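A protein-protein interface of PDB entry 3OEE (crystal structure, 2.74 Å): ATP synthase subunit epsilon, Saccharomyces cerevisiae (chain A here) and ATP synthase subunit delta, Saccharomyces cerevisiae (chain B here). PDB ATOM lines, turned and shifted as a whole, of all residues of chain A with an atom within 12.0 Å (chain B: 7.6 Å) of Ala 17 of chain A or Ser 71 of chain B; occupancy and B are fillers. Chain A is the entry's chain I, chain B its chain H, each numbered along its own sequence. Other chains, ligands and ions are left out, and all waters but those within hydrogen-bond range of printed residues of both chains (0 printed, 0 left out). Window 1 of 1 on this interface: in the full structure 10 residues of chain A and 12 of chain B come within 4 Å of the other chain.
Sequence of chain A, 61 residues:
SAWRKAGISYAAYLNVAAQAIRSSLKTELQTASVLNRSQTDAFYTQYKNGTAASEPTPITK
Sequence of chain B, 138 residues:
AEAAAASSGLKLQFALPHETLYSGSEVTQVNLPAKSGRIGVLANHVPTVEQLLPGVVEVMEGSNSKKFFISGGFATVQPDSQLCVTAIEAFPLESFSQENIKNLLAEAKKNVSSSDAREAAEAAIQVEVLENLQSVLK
Among the printed residues, pairs that only touch across the chains: Leu 14 of chain A with Ser 71 of chain B (3.9 Å), Leu 14 of chain A with Gly 72 of chain B (3.4 Å), Leu 14 of chain A with Ile 88 of chain B (3.4 Å), Val 16 of chain A with Glu 122 of chain B (3.2 Å), Ala 17 of chain A with Ser 71 of chain B (3.7 Å), Ala 18 of chain A with Ile 88 of chain B (3.8 Å), Ala 20 of chain A with Leu 130 of chain B (3.99 Å) and Arg 22 of chain A with Glu 89 of chain B (3.5 Å).
The side-chain carboxylate (OE2) of Glu 89 of chain B sits close to the backbone carbonyl oxygen (O) of Ala 18 of chain A (3.0 Å).
OH of Tyr 10 of chain A is in hydrogen-bond range of O of Gly 73 of chain B, at 3.4 Å.
The side-chain carboxylate (OE1) of Glu 89 of chain B is in salt-bridge range of the guanidinium group (NH1) of Arg 37 of chain A.
O of Gly 73 of chain B lies within hydrogen-bond range of N of Leu 52 of chain B, 2.4 Å away.
The backbone NH (N) of Glu 89 of chain B sits at hydrogen-bond distance from the side-chain hydroxyl (OG) of Ser 71 of chain B (3.2 Å).
The side-chain hydroxyl of Ser 71 of chain B sits at hydrogen-bond distance from the backbone NH of Ile 88 of chain B (3.1 Å).
The backbone NH (N) of Ile 88 of chain B lies within hydrogen-bond range of the backbone carbonyl oxygen (O) of Gly 72 of chain B, 3.4 Å away.
Of the printed residues of chain B, Leu 14 of chain A touches Ser 71, Gly 72 and Ile 88.
Of the printed residues of chain B, Val 16 of chain A touches Glu 122.
Printed residues of chain B within 4 Å of Ala 17 of chain A: Ser 71 (3.7 Å).
Printed residues of chain B within 4 Å of Ala 18 of chain A: Ile 88 (3.8 Å) and Glu 89 (3.0 Å).
Printed residues of chain B within 4 Å of Arg 37 of chain A: Glu 89 (2.7 Å).
No residue of chain A comes within 4 Å of Leu 53 of chain B.
No residue of chain A comes within 4 Å of Gly 55 of chain B.
No residue of chain A comes within 4 Å of Phe 69 of chain B.
No residue of chain A comes within 4 Å of Ile 70 of chain B.
Ser 71 of chain B touches two residues of chain A.
Ala 87 of chain B touches none of the printed residues of chain A.
Ile 88 of chain B touches two residues of chain A.
No residue of chain A comes within 4 Å of Ala 90 of chain B.
No residue of chain A comes within 4 Å of Gln 126 of chain B.
No residue of chain A comes within 4 Å of Val 129 of chain B.
Of the printed residues of chain A, Leu 130 of chain B touches Ala 20.
The nearest residue of chain B that does not touch Ala 17 of chain A is Val 129 of chain B (4.5 Å).
Hydrophobic or aromatic side chains of chain B within 4 Å of the printed part of chain A: Ile 88 and Leu 130.
Along chain B the printed residues that touch a printed residue of chain A span positions 71 to 130.
Of the 19 printed residues of chain A, 8 touch a printed residue of chain B.
Hydrophobic or aromatic side chains of chain A that line the printed part of chain B: Tyr 10, Leu 14, Val 16, Ala 18 and Ala 20.
Among the printed residues, Asp or Glu carboxylates within 4 Å of a Lys or Arg side-chain nitrogen of the other chain: Arg 37 of chain A with Glu 89 of chain B.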
ATOM      1  N   ILE A   8     -17.351 -11.183   9.400  1.00  0.00           N
ATOM      2  CA  ILE A   8     -16.286 -10.189   9.712  1.00  0.00           C
ATOM      3  C   ILE A   8     -16.503  -9.560  11.091  1.00  0.00           C
ATOM      4  O   ILE A   8     -17.643  -9.405  11.538  1.00  0.00           O
ATOM      5  CB  ILE A   8     -16.218  -9.085   8.642  1.00  0.00           C
ATOM      6  N   SER A   9     -15.401  -9.211  11.754  1.00  0.00           N
ATOM      7  CA  SER A   9     -15.423  -8.594  13.090  1.00  0.00           C
ATOM      8  C   SER A   9     -14.399  -7.448  13.185  1.00  0.00           C
ATOM      9  O   SER A   9     -13.544  -7.326  12.308  1.00  0.00           O
ATOM     10  CB  SER A   9     -15.143  -9.645  14.168  1.00  0.00           C
ATOM     11  OG  SER A   9     -13.756  -9.951  14.234  1.00  0.00           O
ATOM     12  N   TYR A  10     -14.480  -6.634  14.249  1.00  0.00           N
ATOM     13  CA  TYR A  10     -13.643  -5.416  14.405  1.00  0.00           C
ATOM     14  C   TYR A  10     -12.142  -5.667  14.277  1.00  0.00           C
ATOM     15  O   TYR A  10     -11.419  -4.824  13.751  1.00  0.00           O
ATOM     16  CB  TYR A  10     -13.946  -4.656  15.715  1.00  0.00           C
ATOM     17  CG  TYR A  10     -13.218  -3.312  15.867  1.00  0.00           C
ATOM     18  CD1 TYR A  10     -13.624  -2.181  15.149  1.00  0.00           C
ATOM     19  CD2 TYR A  10     -12.133  -3.172  16.740  1.00  0.00           C
ATOM     20  CE1 TYR A  10     -12.961  -0.950  15.289  1.00  0.00           C
ATOM     21  CE2 TYR A  10     -11.465  -1.947  16.882  1.00  0.00           C
ATOM     22  CZ  TYR A  10     -11.887  -0.840  16.158  1.00  0.00           C
ATOM     23  OH  TYR A  10     -11.233   0.371  16.296  1.00  0.00           O
ATOM     24  N   ALA A  11     -11.680  -6.816  14.762  1.00  0.00           N
ATOM     25  CA  ALA A  11     -10.297  -7.222  14.539  1.00  0.00           C
ATOM     26  C   ALA A  11     -10.069  -7.517  13.050  1.00  0.00           C
ATOM     27  O   ALA A  11      -9.185  -6.929  12.422  1.00  0.00           O
ATOM     28  CB  ALA A  11      -9.957  -8.433  15.394  1.00  0.00           C
ATOM     29  N   ALA A  12     -10.897  -8.402  12.495  1.00  0.00           N
ATOM     30  CA  ALA A  12     -10.737  -8.896  11.124  1.00  0.00           C
ATOM     31  C   ALA A  12     -11.021  -7.832  10.072  1.00  0.00           C
ATOM     32  O   ALA A  12     -10.411  -7.831   9.005  1.00  0.00           O
ATOM     33  CB  ALA A  12     -11.622 -10.115  10.896  1.00  0.00           C
ATOM     34  N   TYR A  13     -11.965  -6.950  10.378  1.00  0.00           N
ATOM     35  CA  TYR A  13     -12.291  -5.806   9.535  1.00  0.00           C
ATOM     36  C   TYR A  13     -11.049  -4.935   9.377  1.00  0.00           C
ATOM     37  O   TYR A  13     -10.634  -4.628   8.254  1.00  0.00           O
ATOM     38  CB  TYR A  13     -13.481  -5.038  10.144  1.00  0.00           C
ATOM     39  CG  TYR A  13     -13.534  -3.538   9.903  1.00  0.00           C
ATOM     40  CD1 TYR A  13     -13.226  -2.644  10.930  1.00  0.00           C
ATOM     41  CD2 TYR A  13     -13.922  -3.016   8.664  1.00  0.00           C
ATOM     42  CE1 TYR A  13     -13.280  -1.270  10.728  1.00  0.00           C
ATOM     43  CE2 TYR A  13     -13.979  -1.640   8.450  1.00  0.00           C
ATOM     44  CZ  TYR A  13     -13.657  -0.774   9.487  1.00  0.00           C
ATOM     45  OH  TYR A  13     -13.707   0.587   9.288  1.00  0.00           O
ATOM     46  N   LEU A  14     -10.443  -4.584  10.508  1.00  0.00           N
ATOM     47  CA  LEU A  14      -9.234  -3.774  10.521  1.00  0.00           C
ATOM     48  C   LEU A  14      -8.146  -4.373   9.648  1.00  0.00           C
ATOM     49  O   LEU A  14      -7.433  -3.649   8.946  1.00  0.00           O
ATOM     50  CB  LEU A  14      -8.722  -3.585  11.948  1.00  0.00           C
ATOM     51  CG  LEU A  14      -9.274  -2.378  12.703  1.00  0.00           C
ATOM     52  CD1 LEU A  14      -8.618  -2.244  14.074  1.00  0.00           C
ATOM     53  CD2 LEU A  14      -9.094  -1.099  11.881  1.00  0.00           C
ATOM     54  N   ASN A  15      -8.046  -5.702   9.687  1.00  0.00           N
ATOM     55  CA  ASN A  15      -7.073  -6.454   8.893  1.00  0.00           C
ATOM     56  C   ASN A  15      -7.224  -6.272   7.381  1.00  0.00           C
ATOM     57  O   ASN A  15      -6.223  -6.164   6.670  1.00  0.00           O
ATOM     58  CB  ASN A  15      -7.116  -7.940   9.262  1.00  0.00           C
ATOM     59  CG  ASN A  15      -6.133  -8.769   8.460  1.00  0.00           C
ATOM     60  OD1 ASN A  15      -6.532  -9.648   7.696  1.00  0.00           O
ATOM     61  ND2 ASN A  15      -4.842  -8.487   8.623  1.00  0.00           N
ATOM     62  N   VAL A  16      -8.467  -6.233   6.896  1.00  0.00           N
ATOM     63  CA  VAL A  16      -8.723  -6.005   5.463  1.00  0.00           C
ATOM     64  C   VAL A  16      -8.293  -4.587   5.051  1.00  0.00           C
ATOM     65  O   VAL A  16      -7.841  -4.367   3.924  1.00  0.00           O
ATOM     66  CB  VAL A  16     -10.211  -6.242   5.056  1.00  0.00           C
ATOM     67  CG1 VAL A  16     -10.300  -6.659   3.586  1.00  0.00           C
ATOM     68  CG2 VAL A  16     -10.869  -7.297   5.931  1.00  0.00           C
ATOM     69  N   ALA A  17      -8.436  -3.640   5.980  1.00  0.00           N
ATOM     70  CA  ALA A  17      -7.975  -2.266   5.788  1.00  0.00           C
ATOM     71  C   ALA A  17      -6.499  -2.129   6.178  1.00  0.00           C
ATOM     72  O   ALA A  17      -5.942  -1.025   6.197  1.00  0.00           O
ATOM     73  CB  ALA A  17      -8.841  -1.302   6.593  1.00  0.00           C
ATOM     74  N   ALA A  18      -5.882  -3.263   6.498  1.00  0.00           N
ATOM     75  CA  ALA A  18      -4.464  -3.331   6.817  1.00  0.00           C
ATOM     76  C   ALA A  18      -3.761  -4.181   5.764  1.00  0.00           C
ATOM     77  O   ALA A  18      -2.550  -4.415   5.833  1.00  0.00           O
ATOM     78  CB  ALA A  18      -4.262  -3.914   8.212  1.00  0.00           C
ATOM     79  N   GLN A  19      -4.540  -4.641   4.790  1.00  0.00           N
ATOM     80  CA  GLN A  19      -4.030  -5.429   3.675  1.00  0.00           C
ATOM     81  C   GLN A  19      -4.366  -4.714   2.363  1.00  0.00           C
ATOM     82  O   GLN A  19      -3.892  -5.089   1.288  1.00  0.00           O
ATOM     83  CB  GLN A  19      -4.624  -6.838   3.715  1.00  0.00           C
ATOM     84  CG  GLN A  19      -3.587  -7.961   3.629  1.00  0.00           C
ATOM     85  CD  GLN A  19      -3.459  -8.554   2.238  1.00  0.00           C
ATOM     86  OE1 GLN A  19      -3.278  -7.840   1.247  1.00  0.00           O
ATOM     87  NE2 GLN A  19      -3.546  -9.876   2.158  1.00  0.00           N
ATOM     88  N   ALA A  20      -5.202  -3.683   2.473  1.00  0.00           N
ATOM     89  CA  ALA A  20      -5.403  -2.717   1.406  1.00  0.00           C
ATOM     90  C   ALA A  20      -4.341  -1.641   1.574  1.00  0.00           C
ATOM     91  O   ALA A  20      -3.773  -1.160   0.593  1.00  0.00           O
ATOM     92  CB  ALA A  20      -6.793  -2.116   1.482  1.00  0.00           C
ATOM     93  N   ILE A  21      -4.076  -1.279   2.829  1.00  0.00           N
ATOM     94  CA  ILE A  21      -2.970  -0.396   3.172  1.00  0.00           C
ATOM     95  C   ILE A  21      -1.640  -1.046   2.797  1.00  0.00           C
ATOM     96  O   ILE A  21      -0.710  -0.367   2.371  1.00  0.00           O
ATOM     97  CB  ILE A  21      -2.964  -0.047   4.674  1.00  0.00           C
ATOM     98  N   ARG A  22      -1.570  -2.369   2.944  1.00  0.00           N
ATOM     99  CA  ARG A  22      -0.367  -3.136   2.610  1.00  0.00           C
ATOM    100  C   ARG A  22      -0.194  -3.394   1.101  1.00  0.00           C
ATOM    101  O   ARG A  22       0.936  -3.447   0.607  1.00  0.00           O
ATOM    102  CB  ARG A  22      -0.323  -4.450   3.404  1.00  0.00           C
ATOM    103  N   SER A  23      -1.302  -3.547   0.374  1.00  0.00           N
ATOM    104  CA  SER A  23      -1.244  -3.777  -1.074  1.00  0.00           C
ATOM    105  C   SER A  23      -1.767  -2.581  -1.862  1.00  0.00           C
ATOM    106  O   SER A  23      -1.113  -1.541  -1.937  1.00  0.00           O
ATOM    107  CB  SER A  23      -2.014  -5.045  -1.453  1.00  0.00           C
ATOM    108  N   VAL A  34       6.962  -7.126   4.841  1.00  0.00           N
ATOM    109  CA  VAL A  34       5.606  -6.608   4.624  1.00  0.00           C
ATOM    110  C   VAL A  34       4.730  -7.710   4.016  1.00  0.00           C
ATOM    111  O   VAL A  34       3.638  -7.995   4.527  1.00  0.00           O
ATOM    112  CB  VAL A  34       5.601  -5.299   3.772  1.00  0.00           C
ATOM    113  CG1 VAL A  34       4.317  -5.158   2.947  1.00  0.00           C
ATOM    114  CG2 VAL A  34       5.800  -4.085   4.671  1.00  0.00           C
ATOM    115  N   ARG A  37       3.719 -10.432   6.623  1.00  0.00           N
ATOM    116  CA  ARG A  37       2.623 -10.009   7.494  1.00  0.00           C
ATOM    117  C   ARG A  37       1.252 -10.088   6.798  1.00  0.00           C
ATOM    118  O   ARG A  37       0.216 -10.259   7.460  1.00  0.00           O
ATOM    119  CB  ARG A  37       2.935  -8.594   7.999  1.00  0.00           C
ATOM    120  CG  ARG A  37       1.791  -7.790   8.606  1.00  0.00           C
ATOM    121  CD  ARG A  37       2.023  -6.295   8.371  1.00  0.00           C
ATOM    122  NE  ARG A  37       3.428  -5.930   8.559  1.00  0.00           N
ATOM    123  CZ  ARG A  37       3.969  -4.772   8.194  1.00  0.00           C
ATOM    124  NH1 ARG A  37       3.240  -3.831   7.611  1.00  0.00           N
ATOM    125  NH2 ARG A  37       5.253  -4.555   8.415  1.00  0.00           N
ATOM    126  N   SER A  38       1.265  -9.986   5.467  1.00  0.00           N
ATOM    127  CA  SER A  38       0.052 -10.103   4.647  1.00  0.00           C
ATOM    128  C   SER A  38      -0.269 -11.546   4.203  1.00  0.00           C
ATOM    129  O   SER A  38      -1.036 -11.748   3.263  1.00  0.00           O
ATOM    130  CB  SER A  38       0.134  -9.168   3.430  1.00  0.00           C
ATOM    131  OG  SER A  38      -0.209  -7.836   3.770  1.00  0.00           O
ATOM    132  N   LEU B  16       2.270   0.757  16.590  1.00  0.00           N
ATOM    133  CA  LEU B  16       1.832  -0.310  15.694  1.00  0.00           C
ATOM    134  C   LEU B  16       2.471  -1.596  16.205  1.00  0.00           C
ATOM    135  O   LEU B  16       3.537  -1.542  16.833  1.00  0.00           O
ATOM    136  CB  LEU B  16       2.276  -0.052  14.249  1.00  0.00           C
ATOM    137  CG  LEU B  16       1.949   1.253  13.521  1.00  0.00           C
ATOM    138  CD1 LEU B  16       2.644   1.246  12.168  1.00  0.00           C
ATOM    139  CD2 LEU B  16       0.449   1.468  13.357  1.00  0.00           C
ATOM    140  N   PRO B  17       1.837  -2.756  15.941  1.00  0.00           N
ATOM    141  CA  PRO B  17       2.337  -4.030  16.482  1.00  0.00           C
ATOM    142  C   PRO B  17       3.693  -4.469  15.906  1.00  0.00           C
ATOM    143  O   PRO B  17       4.396  -5.265  16.532  1.00  0.00           O
ATOM    144  CB  PRO B  17       1.238  -5.027  16.101  1.00  0.00           C
ATOM    145  CG  PRO B  17       0.552  -4.416  14.913  1.00  0.00           C
ATOM    146  CD  PRO B  17       0.629  -2.936  15.109  1.00  0.00           C
ATOM    147  N   LEU B  52     -10.370   4.720  16.601  1.00  0.00           N
ATOM    148  CA  LEU B  52      -9.810   5.421  15.447  1.00  0.00           C
ATOM    149  C   LEU B  52     -10.200   4.704  14.156  1.00  0.00           C
ATOM    150  O   LEU B  52      -9.837   3.550  13.946  1.00  0.00           O
ATOM    151  CB  LEU B  52      -8.282   5.531  15.562  1.00  0.00           C
ATOM    152  CG  LEU B  52      -7.694   6.193  16.815  1.00  0.00           C
ATOM    153  CD1 LEU B  52      -6.239   5.813  17.015  1.00  0.00           C
ATOM    154  CD2 LEU B  52      -7.847   7.701  16.767  1.00  0.00           C
ATOM    155  N   LEU B  53     -10.976   5.388  13.319  1.00  0.00           N
ATOM    156  CA  LEU B  53     -11.288   4.931  11.966  1.00  0.00           C
ATOM    157  C   LEU B  53     -10.119   5.320  11.049  1.00  0.00           C
ATOM    158  O   LEU B  53      -9.286   6.150  11.438  1.00  0.00           O
ATOM    159  CB  LEU B  53     -12.592   5.578  11.488  1.00  0.00           C
ATOM    160  N   PRO B  54     -10.044   4.731   9.833  1.00  0.00           N
ATOM    161  CA  PRO B  54      -8.993   5.105   8.876  1.00  0.00           C
ATOM    162  C   PRO B  54      -8.836   6.627   8.728  1.00  0.00           C
ATOM    163  O   PRO B  54      -9.836   7.354   8.786  1.00  0.00           O
ATOM    164  CB  PRO B  54      -9.494   4.504   7.561  1.00  0.00           C
ATOM    165  CG  PRO B  54     -10.312   3.340   7.965  1.00  0.00           C
ATOM    166  CD  PRO B  54     -10.922   3.671   9.297  1.00  0.00           C
ATOM    167  N   GLY B  55      -7.599   7.100   8.549  1.00  0.00           N
ATOM    168  CA  GLY B  55      -7.326   8.542   8.415  1.00  0.00           C
ATOM    169  C   GLY B  55      -5.941   8.994   8.855  1.00  0.00           C
ATOM    170  O   GLY B  55      -5.126   8.184   9.308  1.00  0.00           O
ATOM    171  N   VAL B  56      -5.679  10.295   8.725  1.00  0.00           N
ATOM    172  CA  VAL B  56      -4.357  10.868   9.019  1.00  0.00           C
ATOM    173  C   VAL B  56      -4.149  11.206  10.502  1.00  0.00           C
ATOM    174  O   VAL B  56      -5.118  11.353  11.251  1.00  0.00           O
ATOM    175  CB  VAL B  56      -4.096  12.128   8.172  1.00  0.00           C
ATOM    176  N   PHE B  69      -0.480   7.813   8.134  1.00  0.00           N
ATOM    177  CA  PHE B  69      -1.763   7.229   7.731  1.00  0.00           C
ATOM    178  C   PHE B  69      -2.172   6.046   8.614  1.00  0.00           C
ATOM    179  O   PHE B  69      -1.400   5.100   8.800  1.00  0.00           O
ATOM    180  CB  PHE B  69      -1.766   6.820   6.257  1.00  0.00           C
ATOM    181  CG  PHE B  69      -3.107   6.347   5.772  1.00  0.00           C
ATOM    182  CD1 PHE B  69      -4.111   7.262   5.467  1.00  0.00           C
ATOM    183  CD2 PHE B  69      -3.372   4.990   5.632  1.00  0.00           C
ATOM    184  CE1 PHE B  69      -5.357   6.831   5.026  1.00  0.00           C
ATOM    185  CE2 PHE B  69      -4.614   4.546   5.193  1.00  0.00           C
ATOM    186  CZ  PHE B  69      -5.609   5.466   4.889  1.00  0.00           C
ATOM    187  N   ILE B  70      -3.398   6.100   9.129  1.00  0.00           N
ATOM    188  CA  ILE B  70      -3.886   5.098  10.075  1.00  0.00           C
ATOM    189  C   ILE B  70      -4.903   4.136   9.452  1.00  0.00           C
ATOM    190  O   ILE B  70      -5.838   4.559   8.774  1.00  0.00           O
ATOM    191  CB  ILE B  70      -4.424   5.776  11.381  1.00  0.00           C
ATOM    192  CG1 ILE B  70      -3.273   5.959  12.387  1.00  0.00           C
ATOM    193  CG2 ILE B  70      -5.607   5.003  11.989  1.00  0.00           C
ATOM    194  CD1 ILE B  70      -3.702   6.241  13.832  1.00  0.00           C
ATOM    195  N   SER B  71      -4.687   2.841   9.678  1.00  0.00           N
ATOM    196  CA  SER B  71      -5.648   1.797   9.309  1.00  0.00           C
ATOM    197  C   SER B  71      -6.901   1.894  10.181  1.00  0.00           C
ATOM    198  O   SER B  71      -8.024   1.988   9.676  1.00  0.00           O
ATOM    199  CB  SER B  71      -5.021   0.409   9.480  1.00  0.00           C
ATOM    200  OG  SER B  71      -4.744   0.136  10.847  1.00  0.00           O
ATOM    201  N   GLY B  72      -6.678   1.861  11.493  1.00  0.00           N
ATOM    202  CA  GLY B  72      -7.729   1.942  12.507  1.00  0.00           C
ATOM    203  C   GLY B  72      -7.189   1.464  13.844  1.00  0.00           C
ATOM    204  O   GLY B  72      -6.080   0.925  13.913  1.00  0.00           O
ATOM    205  N   GLY B  73      -7.961   1.655  14.911  1.00  0.00           N
ATOM    206  CA  GLY B  73      -7.523   1.230  16.236  1.00  0.00           C
ATOM    207  C   GLY B  73      -8.014   2.135  17.342  1.00  0.00           C
ATOM    208  O   GLY B  73      -9.039   2.790  17.195  1.00  0.00           O
ATOM    209  N   THR B  86      -2.903   3.687  19.105  1.00  0.00           N
ATOM    210  CA  THR B  86      -2.590   2.368  18.549  1.00  0.00           C
ATOM    211  C   THR B  86      -3.381   2.164  17.262  1.00  0.00           C
ATOM    212  O   THR B  86      -4.608   2.257  17.262  1.00  0.00           O
ATOM    213  CB  THR B  86      -2.946   1.199  19.510  1.00  0.00           C
ATOM    214  OG1 THR B  86      -4.327   1.286  19.884  1.00  0.00           O
ATOM    215  CG2 THR B  86      -2.073   1.193  20.761  1.00  0.00           C
ATOM    216  N   ALA B  87      -2.669   1.904  16.172  1.00  0.00           N
ATOM    217  CA  ALA B  87      -3.292   1.464  14.925  1.00  0.00           C
ATOM    218  C   ALA B  87      -2.686   0.122  14.527  1.00  0.00           C
ATOM    219  O   ALA B  87      -1.972  -0.490  15.320  1.00  0.00           O
ATOM    220  CB  ALA B  87      -3.093   2.495  13.832  1.00  0.00           C
ATOM    221  N   ILE B  88      -2.960  -0.344  13.311  1.00  0.00           N
ATOM    222  CA  ILE B  88      -2.335  -1.582  12.828  1.00  0.00           C
ATOM    223  C   ILE B  88      -1.286  -1.331  11.737  1.00  0.00           C
ATOM    224  O   ILE B  88      -0.214  -1.942  11.757  1.00  0.00           O
ATOM    225  CB  ILE B  88      -3.386  -2.628  12.392  1.00  0.00           C
ATOM    226  CG1 ILE B  88      -4.200  -3.075  13.605  1.00  0.00           C
ATOM    227  CG2 ILE B  88      -2.724  -3.845  11.730  1.00  0.00           C
ATOM    228  CD1 ILE B  88      -5.579  -3.490  13.255  1.00  0.00           C
ATOM    229  N   GLU B  89      -1.598  -0.427  10.807  1.00  0.00           N
ATOM    230  CA  GLU B  89      -0.666  -0.007   9.753  1.00  0.00           C
ATOM    231  C   GLU B  89      -0.524   1.515   9.748  1.00  0.00           C
ATOM    232  O   GLU B  89      -1.503   2.229  10.000  1.00  0.00           O
ATOM    233  CB  GLU B  89      -1.151  -0.480   8.371  1.00  0.00           C
ATOM    234  CG  GLU B  89      -1.266  -2.002   8.183  1.00  0.00           C
ATOM    235  CD  GLU B  89       0.033  -2.671   7.738  1.00  0.00           C
ATOM    236  OE1 GLU B  89       1.016  -2.658   8.507  1.00  0.00           O
ATOM    237  OE2 GLU B  89       0.058  -3.226   6.617  1.00  0.00           O
ATOM    238  N   ALA B  90       0.690   2.001   9.466  1.00  0.00           N
ATOM    239  CA  ALA B  90       0.962   3.442   9.304  1.00  0.00           C
ATOM    240  C   ALA B  90       2.210   3.717   8.456  1.00  0.00           C
ATOM    241  O   ALA B  90       2.248   3.412   7.256  1.00  0.00           O
ATOM    242  CB  ALA B  90       1.076   4.143  10.666  1.00  0.00           C
ATOM    243  N   GLU B 122     -15.980  -8.902   2.535  1.00  0.00           N
ATOM    244  CA  GLU B 122     -14.575  -8.566   2.830  1.00  0.00           C
ATOM    245  C   GLU B 122     -13.981  -7.617   1.779  1.00  0.00           C
ATOM    246  O   GLU B 122     -13.186  -6.733   2.110  1.00  0.00           O
ATOM    247  CB  GLU B 122     -13.698  -9.819   3.056  1.00  0.00           C
ATOM    248  CG  GLU B 122     -13.068 -10.449   1.805  1.00  0.00           C
ATOM    249  CD  GLU B 122     -11.867 -11.343   2.113  1.00  0.00           C
ATOM    250  OE1 GLU B 122     -11.134 -11.073   3.092  1.00  0.00           O
ATOM    251  OE2 GLU B 122     -11.645 -12.317   1.360  1.00  0.00           O
ATOM    252  N   ILE B 125     -15.262  -4.073   2.094  1.00  0.00           N
ATOM    253  CA  ILE B 125     -14.481  -3.313   3.066  1.00  0.00           C
ATOM    254  C   ILE B 125     -13.290  -2.635   2.384  1.00  0.00           C
ATOM    255  O   ILE B 125     -12.708  -1.694   2.927  1.00  0.00           O
ATOM    256  CB  ILE B 125     -13.986  -4.205   4.222  1.00  0.00           C
ATOM    257  N   GLN B 126     -12.940  -3.118   1.193  1.00  0.00           N
ATOM    258  CA  GLN B 126     -11.884  -2.516   0.390  1.00  0.00           C
ATOM    259  C   GLN B 126     -12.318  -1.191  -0.251  1.00  0.00           C
ATOM    260  O   GLN B 126     -11.532  -0.245  -0.297  1.00  0.00           O
ATOM    261  CB  GLN B 126     -11.397  -3.497  -0.679  1.00  0.00           C
ATOM    262  N   VAL B 129     -12.603   1.926   2.055  1.00  0.00           N
ATOM    263  CA  VAL B 129     -11.269   2.189   2.609  1.00  0.00           C
ATOM    264  C   VAL B 129     -10.350   2.923   1.630  1.00  0.00           C
ATOM    265  O   VAL B 129      -9.596   3.815   2.032  1.00  0.00           O
ATOM    266  CB  VAL B 129     -10.578   0.889   3.087  1.00  0.00           C
ATOM    267  N   LEU B 130     -10.422   2.547   0.353  1.00  0.00           N
ATOM    268  CA  LEU B 130      -9.578   3.138  -0.686  1.00  0.00           C
ATOM    269  C   LEU B 130      -9.964   4.583  -0.980  1.00  0.00           C
ATOM    270  O   LEU B 130      -9.097   5.412  -1.266  1.00  0.00           O
ATOM    271  CB  LEU B 130      -9.634   2.307  -1.970  1.00  0.00           C
ATOM    272  CG  LEU B 130      -9.372   0.804  -1.849  1.00  0.00           C
ATOM    273  CD1 LEU B 130      -9.558   0.110  -3.192  1.00  0.00           C
ATOM    274  CD2 LEU B 130      -7.995   0.516  -1.262  1.00  0.00           C
